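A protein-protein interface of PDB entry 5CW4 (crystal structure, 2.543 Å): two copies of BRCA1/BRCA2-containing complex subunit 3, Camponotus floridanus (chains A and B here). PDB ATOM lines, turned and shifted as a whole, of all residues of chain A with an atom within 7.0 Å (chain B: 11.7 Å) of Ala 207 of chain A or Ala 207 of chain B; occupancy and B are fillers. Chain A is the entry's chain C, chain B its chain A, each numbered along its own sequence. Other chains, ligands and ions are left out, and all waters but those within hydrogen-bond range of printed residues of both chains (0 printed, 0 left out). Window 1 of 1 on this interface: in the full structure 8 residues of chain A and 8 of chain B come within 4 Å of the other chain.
Of chain A, only Ala 207 and Arg 211 come within 4 Å of Ala 207 of chain B.
No residue of chain B comes within 4 Å of Asn 206 of chain A.
No residue of chain B comes within 4 Å of Val 208 of chain A.
Printed residues of chain A within 4 Å of Ile 203 of chain B: Thr 210 and Ile 214.
Printed residues of chain A within 4 Å of Leu 200 of chain B: Ile 214 (3.7 Å).
The nearest residue of chain A that does not touch Ala 207 of chain B is Thr 210 of chain A (4.1 Å).
Ile 203 of chain A touches Thr 210 of chain B, and with the chains exchanged Thr 210 of chain A touches Ile 203 of chain B.
His 204 of chain A touches Arg 211 of chain B, and with the chains exchanged Arg 211 of chain A touches His 204 of chain B.
Ala 207 of chain B touches its own counterpart, Ala 207 of chain A.
Arg 211 of chain A touches Ala 207 of chain B, but with the chains exchanged Ala 207 of chain A does not touch Arg 211 of chain B (4.1 Å).
Of the 11 pairs that touch across the chains among the printed residues, 9 have their exchanged pair printed and touching as well.
Among the printed residues, merely in contact across the chains: Arg 211 of chain A with His 204 of chain B, Ile 203 of chain A with Thr 210 of chain B, His 204 of chain A with Arg 211 of chain B, Ala 207 of chain A with Ala 207 of chain B, Thr 210 of chain A with Ile 203 of chain B, Ile 203 of chain A with Ile 214 of chain B, Ile 214 of chain A with Leu 200 of chain B, Ile 214 of chain A with His 204 of chain B, Arg 211 of chain A with Ala 207 of chain B, Ile 214 of chain A with Ile 203 of chain B and His 204 of chain A with Ile 214 of chain B.
Hydrophobic or aromatic side chains of chain A within 4 Å of the printed part of chain B: Ile 203, His 204, Ala 207 and Ile 214.
Of the 25 printed residues of chain B, 7 touch a printed residue of chain A.
Printed residues of chain B that touch a printed residue of chain A: Leu 200, Ile 203, His 204, Ala 207, Thr 210, Arg 211 and Ile 214.
Hydrophobic or aromatic side chains of chain B that line the printed part of chain A: Leu 200, Ile 203, His 204, Ala 207 and Ile 214.
Among the printed residues, 11 pairs touch across the chains.
Among the printed residues, no Asp or Glu carboxylate lies within 4 Å of a Lys or Arg side-chain nitrogen of the other chain.
The side-chain carboxylate (OD1) of Asp 198 of chain B is in hydrogen-bond range of the backbone NH (N) of Leu 200 of chain B.
OG1 of Thr 210 of chain B sits at hydrogen-bond distance from O of Asn 206 of chain B (3.1 Å).
The backbone carbonyl oxygen (O) of Asn 206 of chain A is in hydrogen-bond range of the side-chain hydroxyl (OG1) of Thr 210 of chain A, at 2.8 Å.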
ATOM      1  N   ALA A 201       1.007 -25.670  -3.474  1.00  0.00           N
ATOM      2  CA  ALA A 201       0.166 -24.645  -4.080  1.00  0.00           C
ATOM      3  C   ALA A 201      -1.309 -24.930  -3.809  1.00  0.00           C
ATOM      4  O   ALA A 201      -2.064 -24.047  -3.390  1.00  0.00           O
ATOM      5  CB  ALA A 201       0.424 -24.563  -5.574  1.00  0.00           C
ATOM      6  N   SER A 202      -1.711 -26.174  -4.049  1.00  0.00           N
ATOM      7  CA  SER A 202      -3.091 -26.588  -3.850  1.00  0.00           C
ATOM      8  C   SER A 202      -3.546 -26.342  -2.413  1.00  0.00           C
ATOM      9  O   SER A 202      -4.631 -25.805  -2.182  1.00  0.00           O
ATOM     10  CB  SER A 202      -3.260 -28.067  -4.218  1.00  0.00           C
ATOM     11  OG  SER A 202      -4.516 -28.557  -3.775  1.00  0.00           O
ATOM     12  N   ILE A 203      -2.716 -26.727  -1.450  1.00  0.00           N
ATOM     13  CA  ILE A 203      -3.058 -26.541  -0.043  1.00  0.00           C
ATOM     14  C   ILE A 203      -3.080 -25.059   0.311  1.00  0.00           C
ATOM     15  O   ILE A 203      -3.900 -24.612   1.115  1.00  0.00           O
ATOM     16  CB  ILE A 203      -2.073 -27.270   0.882  1.00  0.00           C
ATOM     17  CG1 ILE A 203      -2.097 -28.771   0.593  1.00  0.00           C
ATOM     18  CG2 ILE A 203      -2.420 -26.998   2.341  1.00  0.00           C
ATOM     19  CD1 ILE A 203      -1.074 -29.568   1.377  1.00  0.00           C
ATOM     20  N   HIS A 204      -2.172 -24.305  -0.299  1.00  0.00           N
ATOM     21  CA  HIS A 204      -2.124 -22.862  -0.122  1.00  0.00           C
ATOM     22  C   HIS A 204      -3.404 -22.198  -0.622  1.00  0.00           C
ATOM     23  O   HIS A 204      -4.068 -21.471   0.121  1.00  0.00           O
ATOM     24  CB  HIS A 204      -0.916 -22.273  -0.848  1.00  0.00           C
ATOM     25  CG  HIS A 204      -0.876 -20.779  -0.831  1.00  0.00           C
ATOM     26  ND1 HIS A 204      -0.222 -20.062   0.149  1.00  0.00           N
ATOM     27  CD2 HIS A 204      -1.418 -19.864  -1.669  1.00  0.00           C
ATOM     28  CE1 HIS A 204      -0.359 -18.770  -0.090  1.00  0.00           C
ATOM     29  NE2 HIS A 204      -1.082 -18.623  -1.186  1.00  0.00           N
ATOM     30  N   ASN A 205      -3.743 -22.453  -1.883  1.00  0.00           N
ATOM     31  CA  ASN A 205      -4.917 -21.841  -2.497  1.00  0.00           C
ATOM     32  C   ASN A 205      -6.204 -22.136  -1.729  1.00  0.00           C
ATOM     33  O   ASN A 205      -7.063 -21.265  -1.591  1.00  0.00           O
ATOM     34  CB  ASN A 205      -5.058 -22.297  -3.953  1.00  0.00           C
ATOM     35  CG  ASN A 205      -3.975 -21.728  -4.850  1.00  0.00           C
ATOM     36  OD1 ASN A 205      -3.362 -20.709  -4.530  1.00  0.00           O
ATOM     37  ND2 ASN A 205      -3.739 -22.379  -5.983  1.00  0.00           N
ATOM     38  N   ASN A 206      -6.333 -23.358  -1.219  1.00  0.00           N
ATOM     39  CA  ASN A 206      -7.507 -23.725  -0.430  1.00  0.00           C
ATOM     40  C   ASN A 206      -7.554 -22.997   0.908  1.00  0.00           C
ATOM     41  O   ASN A 206      -8.621 -22.585   1.361  1.00  0.00           O
ATOM     42  CB  ASN A 206      -7.550 -25.235  -0.201  1.00  0.00           C
ATOM     43  CG  ASN A 206      -7.972 -25.992  -1.436  1.00  0.00           C
ATOM     44  OD1 ASN A 206      -8.750 -25.490  -2.246  1.00  0.00           O
ATOM     45  ND2 ASN A 206      -7.459 -27.205  -1.592  1.00  0.00           N
ATOM     46  N   ALA A 207      -6.394 -22.844   1.537  1.00  0.00           N
ATOM     47  CA  ALA A 207      -6.298 -22.086   2.776  1.00  0.00           C
ATOM     48  C   ALA A 207      -6.646 -20.625   2.522  1.00  0.00           C
ATOM     49  O   ALA A 207      -7.385 -20.014   3.295  1.00  0.00           O
ATOM     50  CB  ALA A 207      -4.906 -22.207   3.373  1.00  0.00           C
ATOM     51  N   VAL A 208      -6.109 -20.073   1.435  1.00  0.00           N
ATOM     52  CA  VAL A 208      -6.404 -18.697   1.050  1.00  0.00           C
ATOM     53  C   VAL A 208      -7.902 -18.515   0.828  1.00  0.00           C
ATOM     54  O   VAL A 208      -8.514 -17.586   1.357  1.00  0.00           O
ATOM     55  CB  VAL A 208      -5.649 -18.283  -0.235  1.00  0.00           C
ATOM     56  CG1 VAL A 208      -6.246 -17.015  -0.819  1.00  0.00           C
ATOM     57  CG2 VAL A 208      -4.163 -18.103   0.045  1.00  0.00           C
ATOM     58  N   ARG A 209      -8.492 -19.419   0.053  1.00  0.00           N
ATOM     59  CA  ARG A 209      -9.912 -19.341  -0.263  1.00  0.00           C
ATOM     60  C   ARG A 209     -10.786 -19.515   0.980  1.00  0.00           C
ATOM     61  O   ARG A 209     -11.829 -18.872   1.111  1.00  0.00           O
ATOM     62  CB  ARG A 209     -10.274 -20.388  -1.310  1.00  0.00           C
ATOM     63  CG  ARG A 209     -11.729 -20.365  -1.738  1.00  0.00           C
ATOM     64  CD  ARG A 209     -12.032 -21.537  -2.652  1.00  0.00           C
ATOM     65  NE  ARG A 209     -13.459 -21.652  -2.936  1.00  0.00           N
ATOM     66  CZ  ARG A 209     -14.001 -22.658  -3.612  1.00  0.00           C
ATOM     67  NH1 ARG A 209     -13.235 -23.639  -4.069  1.00  0.00           N
ATOM     68  NH2 ARG A 209     -15.307 -22.688  -3.827  1.00  0.00           N
ATOM     69  N   THR A 210     -10.358 -20.385   1.890  1.00  0.00           N
ATOM     70  CA  THR A 210     -11.103 -20.618   3.123  1.00  0.00           C
ATOM     71  C   THR A 210     -11.130 -19.377   4.008  1.00  0.00           C
ATOM     72  O   THR A 210     -12.155 -19.044   4.598  1.00  0.00           O
ATOM     73  CB  THR A 210     -10.515 -21.787   3.926  1.00  0.00           C
ATOM     74  OG1 THR A 210     -10.701 -23.007   3.196  1.00  0.00           O
ATOM     75  CG2 THR A 210     -11.205 -21.904   5.280  1.00  0.00           C
ATOM     76  N   ARG A 211      -9.996 -18.692   4.100  1.00  0.00           N
ATOM     77  CA  ARG A 211      -9.918 -17.487   4.908  1.00  0.00           C
ATOM     78  C   ARG A 211     -10.773 -16.382   4.302  1.00  0.00           C
ATOM     79  O   ARG A 211     -11.404 -15.612   5.025  1.00  0.00           O
ATOM     80  CB  ARG A 211      -8.471 -17.020   5.046  1.00  0.00           C
ATOM     81  CG  ARG A 211      -8.296 -15.816   5.950  1.00  0.00           C
ATOM     82  CD  ARG A 211      -6.896 -15.251   5.830  1.00  0.00           C
ATOM     83  NE  ARG A 211      -6.692 -14.108   6.712  1.00  0.00           N
ATOM     84  CZ  ARG A 211      -5.537 -13.465   6.844  1.00  0.00           C
ATOM     85  NH1 ARG A 211      -4.478 -13.854   6.148  1.00  0.00           N
ATOM     86  NH2 ARG A 211      -5.442 -12.435   7.675  1.00  0.00           N
ATOM     87  N   ALA A 212     -10.793 -16.313   2.975  1.00  0.00           N
ATOM     88  CA  ALA A 212     -11.550 -15.279   2.273  1.00  0.00           C
ATOM     89  C   ALA A 212     -13.053 -15.415   2.501  1.00  0.00           C
ATOM     90  O   ALA A 212     -13.742 -14.424   2.722  1.00  0.00           O
ATOM     91  CB  ALA A 212     -11.243 -15.319   0.789  1.00  0.00           C
ATOM     92  N   ILE A 214     -14.700 -17.095   5.042  1.00  0.00           N
ATOM     93  CA  ILE A 214     -15.024 -16.855   6.441  1.00  0.00           C
ATOM     94  C   ILE A 214     -14.889 -15.371   6.768  1.00  0.00           C
ATOM     95  O   ILE A 214     -15.512 -14.875   7.706  1.00  0.00           O
ATOM     96  CB  ILE A 214     -14.122 -17.681   7.379  1.00  0.00           C
ATOM     97  CG1 ILE A 214     -14.966 -18.639   8.219  1.00  0.00           C
ATOM     98  CG2 ILE A 214     -13.309 -16.772   8.282  1.00  0.00           C
ATOM     99  CD1 ILE A 214     -15.795 -19.601   7.401  1.00  0.00           C
ATOM    100  N   GLU B 186       5.741 -19.934  14.347  1.00  0.00           N
ATOM    101  CA  GLU B 186       4.349 -20.004  13.925  1.00  0.00           C
ATOM    102  C   GLU B 186       3.519 -20.796  14.928  1.00  0.00           C
ATOM    103  O   GLU B 186       2.431 -20.373  15.316  1.00  0.00           O
ATOM    104  CB  GLU B 186       4.234 -20.632  12.535  1.00  0.00           C
ATOM    105  CG  GLU B 186       2.909 -20.336  11.865  1.00  0.00           C
ATOM    106  CD  GLU B 186       2.685 -18.849  11.690  1.00  0.00           C
ATOM    107  OE1 GLU B 186       1.526 -18.403  11.804  1.00  0.00           O
ATOM    108  OE2 GLU B 186       3.672 -18.125  11.437  1.00  0.00           O
ATOM    109  N   GLU B 187       4.042 -21.946  15.342  1.00  0.00           N
ATOM    110  CA  GLU B 187       3.380 -22.775  16.342  1.00  0.00           C
ATOM    111  C   GLU B 187       3.054 -21.984  17.605  1.00  0.00           C
ATOM    112  O   GLU B 187       1.945 -22.080  18.132  1.00  0.00           O
ATOM    113  CB  GLU B 187       4.250 -23.981  16.696  1.00  0.00           C
ATOM    114  CG  GLU B 187       4.397 -24.981  15.576  1.00  0.00           C
ATOM    115  CD  GLU B 187       3.078 -25.612  15.195  1.00  0.00           C
ATOM    116  OE1 GLU B 187       2.284 -25.925  16.107  1.00  0.00           O
ATOM    117  OE2 GLU B 187       2.831 -25.789  13.983  1.00  0.00           O
ATOM    118  N   ALA B 190       0.124 -19.539  16.917  1.00  0.00           N
ATOM    119  CA  ALA B 190      -1.128 -20.274  16.778  1.00  0.00           C
ATOM    120  C   ALA B 190      -1.542 -20.894  18.112  1.00  0.00           C
ATOM    121  O   ALA B 190      -2.729 -21.070  18.382  1.00  0.00           O
ATOM    122  CB  ALA B 190      -0.998 -21.348  15.700  1.00  0.00           C
ATOM    123  N   CYS B 193      -3.947 -19.009  20.545  1.00  0.00           N
ATOM    124  CA  CYS B 193      -5.355 -18.867  20.185  1.00  0.00           C
ATOM    125  C   CYS B 193      -6.031 -20.214  19.942  1.00  0.00           C
ATOM    126  O   CYS B 193      -7.079 -20.286  19.300  1.00  0.00           O
ATOM    127  CB  CYS B 193      -5.497 -17.978  18.947  1.00  0.00           C
ATOM    128  SG  CYS B 193      -4.688 -18.620  17.476  1.00  0.00           S
ATOM    129  N   LYS B 194      -5.431 -21.278  20.463  1.00  0.00           N
ATOM    130  CA  LYS B 194      -6.019 -22.608  20.355  1.00  0.00           C
ATOM    131  C   LYS B 194      -7.348 -22.675  21.100  1.00  0.00           C
ATOM    132  O   LYS B 194      -7.600 -21.883  22.010  1.00  0.00           O
ATOM    133  CB  LYS B 194      -5.063 -23.667  20.907  1.00  0.00           C
ATOM    134  CG  LYS B 194      -4.957 -23.663  22.426  1.00  0.00           C
ATOM    135  CD  LYS B 194      -4.119 -24.829  22.928  1.00  0.00           C
ATOM    136  CE  LYS B 194      -4.120 -24.905  24.448  1.00  0.00           C
ATOM    137  NZ  LYS B 194      -3.468 -23.724  25.076  1.00  0.00           N
ATOM    138  N   HIS B 196     -10.488 -21.984  20.223  1.00  0.00           N
ATOM    139  CA  HIS B 196     -11.370 -20.830  20.114  1.00  0.00           C
ATOM    140  C   HIS B 196     -12.817 -21.300  20.019  1.00  0.00           C
ATOM    141  O   HIS B 196     -13.146 -22.137  19.177  1.00  0.00           O
ATOM    142  CB  HIS B 196     -11.000 -19.971  18.903  1.00  0.00           C
ATOM    143  CG  HIS B 196     -11.497 -18.561  18.991  1.00  0.00           C
ATOM    144  ND1 HIS B 196     -12.828 -18.250  19.182  1.00  0.00           N
ATOM    145  CD2 HIS B 196     -10.842 -17.379  18.919  1.00  0.00           C
ATOM    146  CE1 HIS B 196     -12.970 -16.937  19.222  1.00  0.00           C
ATOM    147  NE2 HIS B 196     -11.779 -16.385  19.065  1.00  0.00           N
ATOM    148  N   ASP B 198     -15.517 -19.761  19.033  1.00  0.00           N
ATOM    149  CA  ASP B 198     -16.207 -19.341  17.817  1.00  0.00           C
ATOM    150  C   ASP B 198     -15.781 -20.211  16.635  1.00  0.00           C
ATOM    151  O   ASP B 198     -14.595 -20.303  16.319  1.00  0.00           O
ATOM    152  CB  ASP B 198     -15.927 -17.863  17.524  1.00  0.00           C
ATOM    153  CG  ASP B 198     -16.912 -17.259  16.533  1.00  0.00           C
ATOM    154  OD1 ASP B 198     -17.446 -18.000  15.682  1.00  0.00           O
ATOM    155  OD2 ASP B 198     -17.152 -16.035  16.604  1.00  0.00           O
ATOM    156  N   VAL B 199     -16.755 -20.845  15.986  1.00  0.00           N
ATOM    157  CA  VAL B 199     -16.476 -21.720  14.849  1.00  0.00           C
ATOM    158  C   VAL B 199     -15.845 -20.954  13.688  1.00  0.00           C
ATOM    159  O   VAL B 199     -14.939 -21.459  13.020  1.00  0.00           O
ATOM    160  CB  VAL B 199     -17.756 -22.419  14.346  1.00  0.00           C
ATOM    161  CG1 VAL B 199     -17.444 -23.288  13.139  1.00  0.00           C
ATOM    162  CG2 VAL B 199     -18.373 -23.252  15.451  1.00  0.00           C
ATOM    163  N   LEU B 200     -16.324 -19.736  13.453  1.00  0.00           N
ATOM    164  CA  LEU B 200     -15.801 -18.911  12.368  1.00  0.00           C
ATOM    165  C   LEU B 200     -14.343 -18.539  12.612  1.00  0.00           C
ATOM    166  O   LEU B 200     -13.549 -18.467  11.675  1.00  0.00           O
ATOM    167  CB  LEU B 200     -16.646 -17.647  12.197  1.00  0.00           C
ATOM    168  CG  LEU B 200     -18.086 -17.862  11.715  1.00  0.00           C
ATOM    169  CD1 LEU B 200     -18.832 -16.546  11.627  1.00  0.00           C
ATOM    170  CD2 LEU B 200     -18.102 -18.568  10.371  1.00  0.00           C
ATOM    171  N   ALA B 201     -13.993 -18.317  13.874  1.00  0.00           N
ATOM    172  CA  ALA B 201     -12.641 -17.898  14.223  1.00  0.00           C
ATOM    173  C   ALA B 201     -11.650 -19.062  14.189  1.00  0.00           C
ATOM    174  O   ALA B 201     -10.490 -18.887  13.817  1.00  0.00           O
ATOM    175  CB  ALA B 201     -12.632 -17.236  15.594  1.00  0.00           C
ATOM    176  N   SER B 202     -12.103 -20.249  14.579  1.00  0.00           N
ATOM    177  CA  SER B 202     -11.231 -21.416  14.570  1.00  0.00           C
ATOM    178  C   SER B 202     -10.933 -21.844  13.136  1.00  0.00           C
ATOM    179  O   SER B 202      -9.808 -22.229  12.813  1.00  0.00           O
ATOM    180  CB  SER B 202     -11.856 -22.569  15.351  1.00  0.00           C
ATOM    181  OG  SER B 202     -13.034 -23.030  14.716  1.00  0.00           O
ATOM    182  N   ILE B 203     -11.947 -21.773  12.280  1.00  0.00           N
ATOM    183  CA  ILE B 203     -11.765 -22.036  10.857  1.00  0.00           C
ATOM    184  C   ILE B 203     -10.804 -21.022  10.258  1.00  0.00           C
ATOM    185  O   ILE B 203      -9.925 -21.373   9.472  1.00  0.00           O
ATOM    186  CB  ILE B 203     -13.099 -21.988  10.095  1.00  0.00           C
ATOM    187  CG1 ILE B 203     -13.983 -23.167  10.499  1.00  0.00           C
ATOM    188  CG2 ILE B 203     -12.857 -21.999   8.595  1.00  0.00           C
ATOM    189  CD1 ILE B 203     -15.338 -23.166   9.837  1.00  0.00           C
ATOM    190  N   HIS B 204     -10.976 -19.761  10.639  1.00  0.00           N
ATOM    191  CA  HIS B 204     -10.074 -18.695  10.218  1.00  0.00           C
ATOM    192  C   HIS B 204      -8.640 -18.988  10.641  1.00  0.00           C
ATOM    193  O   HIS B 204      -7.726 -18.957   9.820  1.00  0.00           O
ATOM    194  CB  HIS B 204     -10.525 -17.352  10.797  1.00  0.00           C
ATOM    195  CG  HIS B 204      -9.521 -16.253  10.630  1.00  0.00           C
ATOM    196  ND1 HIS B 204      -9.527 -15.398   9.548  1.00  0.00           N
ATOM    197  CD2 HIS B 204      -8.478 -15.872  11.404  1.00  0.00           C
ATOM    198  CE1 HIS B 204      -8.532 -14.537   9.665  1.00  0.00           C
ATOM    199  NE2 HIS B 204      -7.878 -14.803  10.783  1.00  0.00           N
ATOM    200  N   ASN B 205      -8.452 -19.274  11.926  1.00  0.00           N
ATOM    201  CA  ASN B 205      -7.119 -19.505  12.477  1.00  0.00           C
ATOM    202  C   ASN B 205      -6.412 -20.690  11.833  1.00  0.00           C
ATOM    203  O   ASN B 205      -5.216 -20.622  11.542  1.00  0.00           O
ATOM    204  CB  ASN B 205      -7.196 -19.704  13.990  1.00  0.00           C
ATOM    205  CG  ASN B 205      -7.521 -18.422  14.728  1.00  0.00           C
ATOM    206  OD1 ASN B 205      -7.116 -17.333  14.312  1.00  0.00           O
ATOM    207  ND2 ASN B 205      -8.257 -18.541  15.831  1.00  0.00           N
ATOM    208  N   ASN B 206      -7.150 -21.774  11.610  1.00  0.00           N
ATOM    209  CA  ASN B 206      -6.606 -22.929  10.903  1.00  0.00           C
ATOM    210  C   ASN B 206      -6.168 -22.567   9.487  1.00  0.00           C
ATOM    211  O   ASN B 206      -5.104 -22.982   9.031  1.00  0.00           O
ATOM    212  CB  ASN B 206      -7.625 -24.062  10.866  1.00  0.00           C
ATOM    213  CG  ASN B 206      -7.895 -24.645  12.236  1.00  0.00           C
ATOM    214  OD1 ASN B 206      -6.997 -24.736  13.070  1.00  0.00           O
ATOM    215  ND2 ASN B 206      -9.140 -25.039  12.479  1.00  0.00           N
ATOM    216  N   ALA B 207      -6.989 -21.780   8.801  1.00  0.00           N
ATOM    217  CA  ALA B 207      -6.642 -21.308   7.468  1.00  0.00           C
ATOM    218  C   ALA B 207      -5.343 -20.506   7.506  1.00  0.00           C
ATOM    219  O   ALA B 207      -4.467 -20.682   6.656  1.00  0.00           O
ATOM    220  CB  ALA B 207      -7.770 -20.475   6.884  1.00  0.00           C
ATOM    221  N   VAL B 208      -5.216 -19.639   8.504  1.00  0.00           N
ATOM    222  CA  VAL B 208      -4.016 -18.820   8.654  1.00  0.00           C
ATOM    223  C   VAL B 208      -2.788 -19.687   8.936  1.00  0.00           C
ATOM    224  O   VAL B 208      -1.724 -19.489   8.345  1.00  0.00           O
ATOM    225  CB  VAL B 208      -4.184 -17.779   9.782  1.00  0.00           C
ATOM    226  CG1 VAL B 208      -2.856 -17.118  10.108  1.00  0.00           C
ATOM    227  CG2 VAL B 208      -5.225 -16.737   9.395  1.00  0.00           C
ATOM    228  N   ARG B 209      -2.946 -20.657   9.831  1.00  0.00           N
ATOM    229  CA  ARG B 209      -1.843 -21.518  10.228  1.00  0.00           C
ATOM    230  C   ARG B 209      -1.365 -22.395   9.073  1.00  0.00           C
ATOM    231  O   ARG B 209      -0.162 -22.558   8.860  1.00  0.00           O
ATOM    232  CB  ARG B 209      -2.247 -22.394  11.422  1.00  0.00           C
ATOM    233  CG  ARG B 209      -1.078 -23.143  12.056  1.00  0.00           C
ATOM    234  CD  ARG B 209      -1.511 -23.949  13.276  1.00  0.00           C
ATOM    235  NE  ARG B 209      -1.640 -25.368  12.961  1.00  0.00           N
ATOM    236  CZ  ARG B 209      -0.661 -26.253  13.110  1.00  0.00           C
ATOM    237  NH1 ARG B 209       0.513 -25.860  13.581  1.00  0.00           N
ATOM    238  NH2 ARG B 209      -0.854 -27.528  12.796  1.00  0.00           N
ATOM    239  N   THR B 210      -2.310 -22.962   8.332  1.00  0.00           N
ATOM    240  CA  THR B 210      -1.972 -23.843   7.218  1.00  0.00           C
ATOM    241  C   THR B 210      -1.226 -23.081   6.123  1.00  0.00           C
ATOM    242  O   THR B 210      -0.266 -23.590   5.551  1.00  0.00           O
ATOM    243  CB  THR B 210      -3.230 -24.509   6.626  1.00  0.00           C
ATOM    244  OG1 THR B 210      -3.819 -25.367   7.611  1.00  0.00           O
ATOM    245  CG2 THR B 210      -2.880 -25.330   5.393  1.00  0.00           C
ATOM    246  N   ARG B 211      -1.661 -21.856   5.848  1.00  0.00           N
ATOM    247  CA  ARG B 211      -1.009 -21.026   4.842  1.00  0.00           C
ATOM    248  C   ARG B 211       0.402 -20.601   5.256  1.00  0.00           C
ATOM    249  O   ARG B 211       1.314 -20.545   4.426  1.00  0.00           O
ATOM    250  CB  ARG B 211      -1.841 -19.781   4.548  1.00  0.00           C
ATOM    251  CG  ARG B 211      -1.123 -18.804   3.636  1.00  0.00           C
ATOM    252  CD  ARG B 211      -1.847 -17.483   3.523  1.00  0.00           C
ATOM    253  NE  ARG B 211      -1.193 -16.605   2.559  1.00  0.00           N
ATOM    254  CZ  ARG B 211      -1.721 -15.476   2.103  1.00  0.00           C
ATOM    255  NH1 ARG B 211      -2.915 -15.086   2.527  1.00  0.00           N
ATOM    256  NH2 ARG B 211      -1.058 -14.742   1.219  1.00  0.00           N
ATOM    257  N   ALA B 212       0.578 -20.282   6.534  1.00  0.00           N
ATOM    258  CA  ALA B 212       1.885 -19.864   7.026  1.00  0.00           C
ATOM    259  C   ALA B 212       2.876 -21.022   6.996  1.00  0.00           C
ATOM    260  O   ALA B 212       4.033 -20.846   6.619  1.00  0.00           O
ATOM    261  CB  ALA B 212       1.772 -19.302   8.430  1.00  0.00           C
ATOM    262  N   LEU B 213       2.420 -22.206   7.394  1.00  0.00           N
ATOM    263  CA  LEU B 213       3.279 -23.383   7.404  1.00  0.00           C
ATOM    264  C   LEU B 213       3.676 -23.784   5.985  1.00  0.00           C
ATOM    265  O   LEU B 213       4.855 -24.011   5.706  1.00  0.00           O
ATOM    266  CB  LEU B 213       2.591 -24.552   8.112  1.00  0.00           C
ATOM    267  CG  LEU B 213       2.470 -24.427   9.633  1.00  0.00           C
ATOM    268  CD1 LEU B 213       1.727 -25.620  10.216  1.00  0.00           C
ATOM    269  CD2 LEU B 213       3.844 -24.283  10.279  1.00  0.00           C
ATOM    270  N   ILE B 214       2.689 -23.867   5.097  1.00  0.00           N
ATOM    271  CA  ILE B 214       2.947 -24.164   3.692  1.00  0.00           C
ATOM    272  C   ILE B 214       3.930 -23.155   3.107  1.00  0.00           C
ATOM    273  O   ILE B 214       4.802 -23.509   2.321  1.00  0.00           O
ATOM    274  CB  ILE B 214       1.643 -24.164   2.864  1.00  0.00           C
ATOM    275  CG1 ILE B 214       0.948 -25.516   2.984  1.00  0.00           C
ATOM    276  CG2 ILE B 214       1.936 -23.899   1.408  1.00  0.00           C
ATOM    277  CD1 ILE B 214       1.779 -26.669   2.458  1.00  0.00           C
ATOM    278  N   HIS B 215       3.782 -21.897   3.509  1.00  0.00           N
ATOM    279  CA  HIS B 215       4.664 -20.817   3.069  1.00  0.00           C
ATOM    280  C   HIS B 215       6.132 -21.122   3.370  1.00  0.00           C
ATOM    281  O   HIS B 215       6.991 -21.006   2.500  1.00  0.00           O
ATOM    282  CB  HIS B 215       4.255 -19.503   3.736  1.00  0.00           C
ATOM    283  CG  HIS B 215       4.940 -18.299   3.171  1.00  0.00           C
ATOM    284  ND1 HIS B 215       5.075 -18.089   1.814  1.00  0.00           N
ATOM    285  CD2 HIS B 215       5.523 -17.238   3.777  1.00  0.00           C
ATOM    286  CE1 HIS B 215       5.716 -16.953   1.610  1.00  0.00           C
ATOM    287  NE2 HIS B 215       5.996 -16.415   2.785  1.00  0.00           N
ATOM    288  N   ILE B 216       6.402 -21.519   4.608  1.00  0.00           N
ATOM    289  CA  ILE B 216       7.742 -21.899   5.036  1.00  0.00           C
ATOM    290  C   ILE B 216       8.277 -23.087   4.236  1.00  0.00           C
ATOM    291  O   ILE B 216       9.408 -23.063   3.750  1.00  0.00           O
ATOM    292  CB  ILE B 216       7.761 -22.247   6.541  1.00  0.00           C
ATOM    293  CG1 ILE B 216       7.405 -21.012   7.376  1.00  0.00           C
ATOM    294  CG2 ILE B 216       9.118 -22.811   6.948  1.00  0.00           C
ATOM    295  CD1 ILE B 216       7.096 -21.320   8.837  1.00  0.00           C
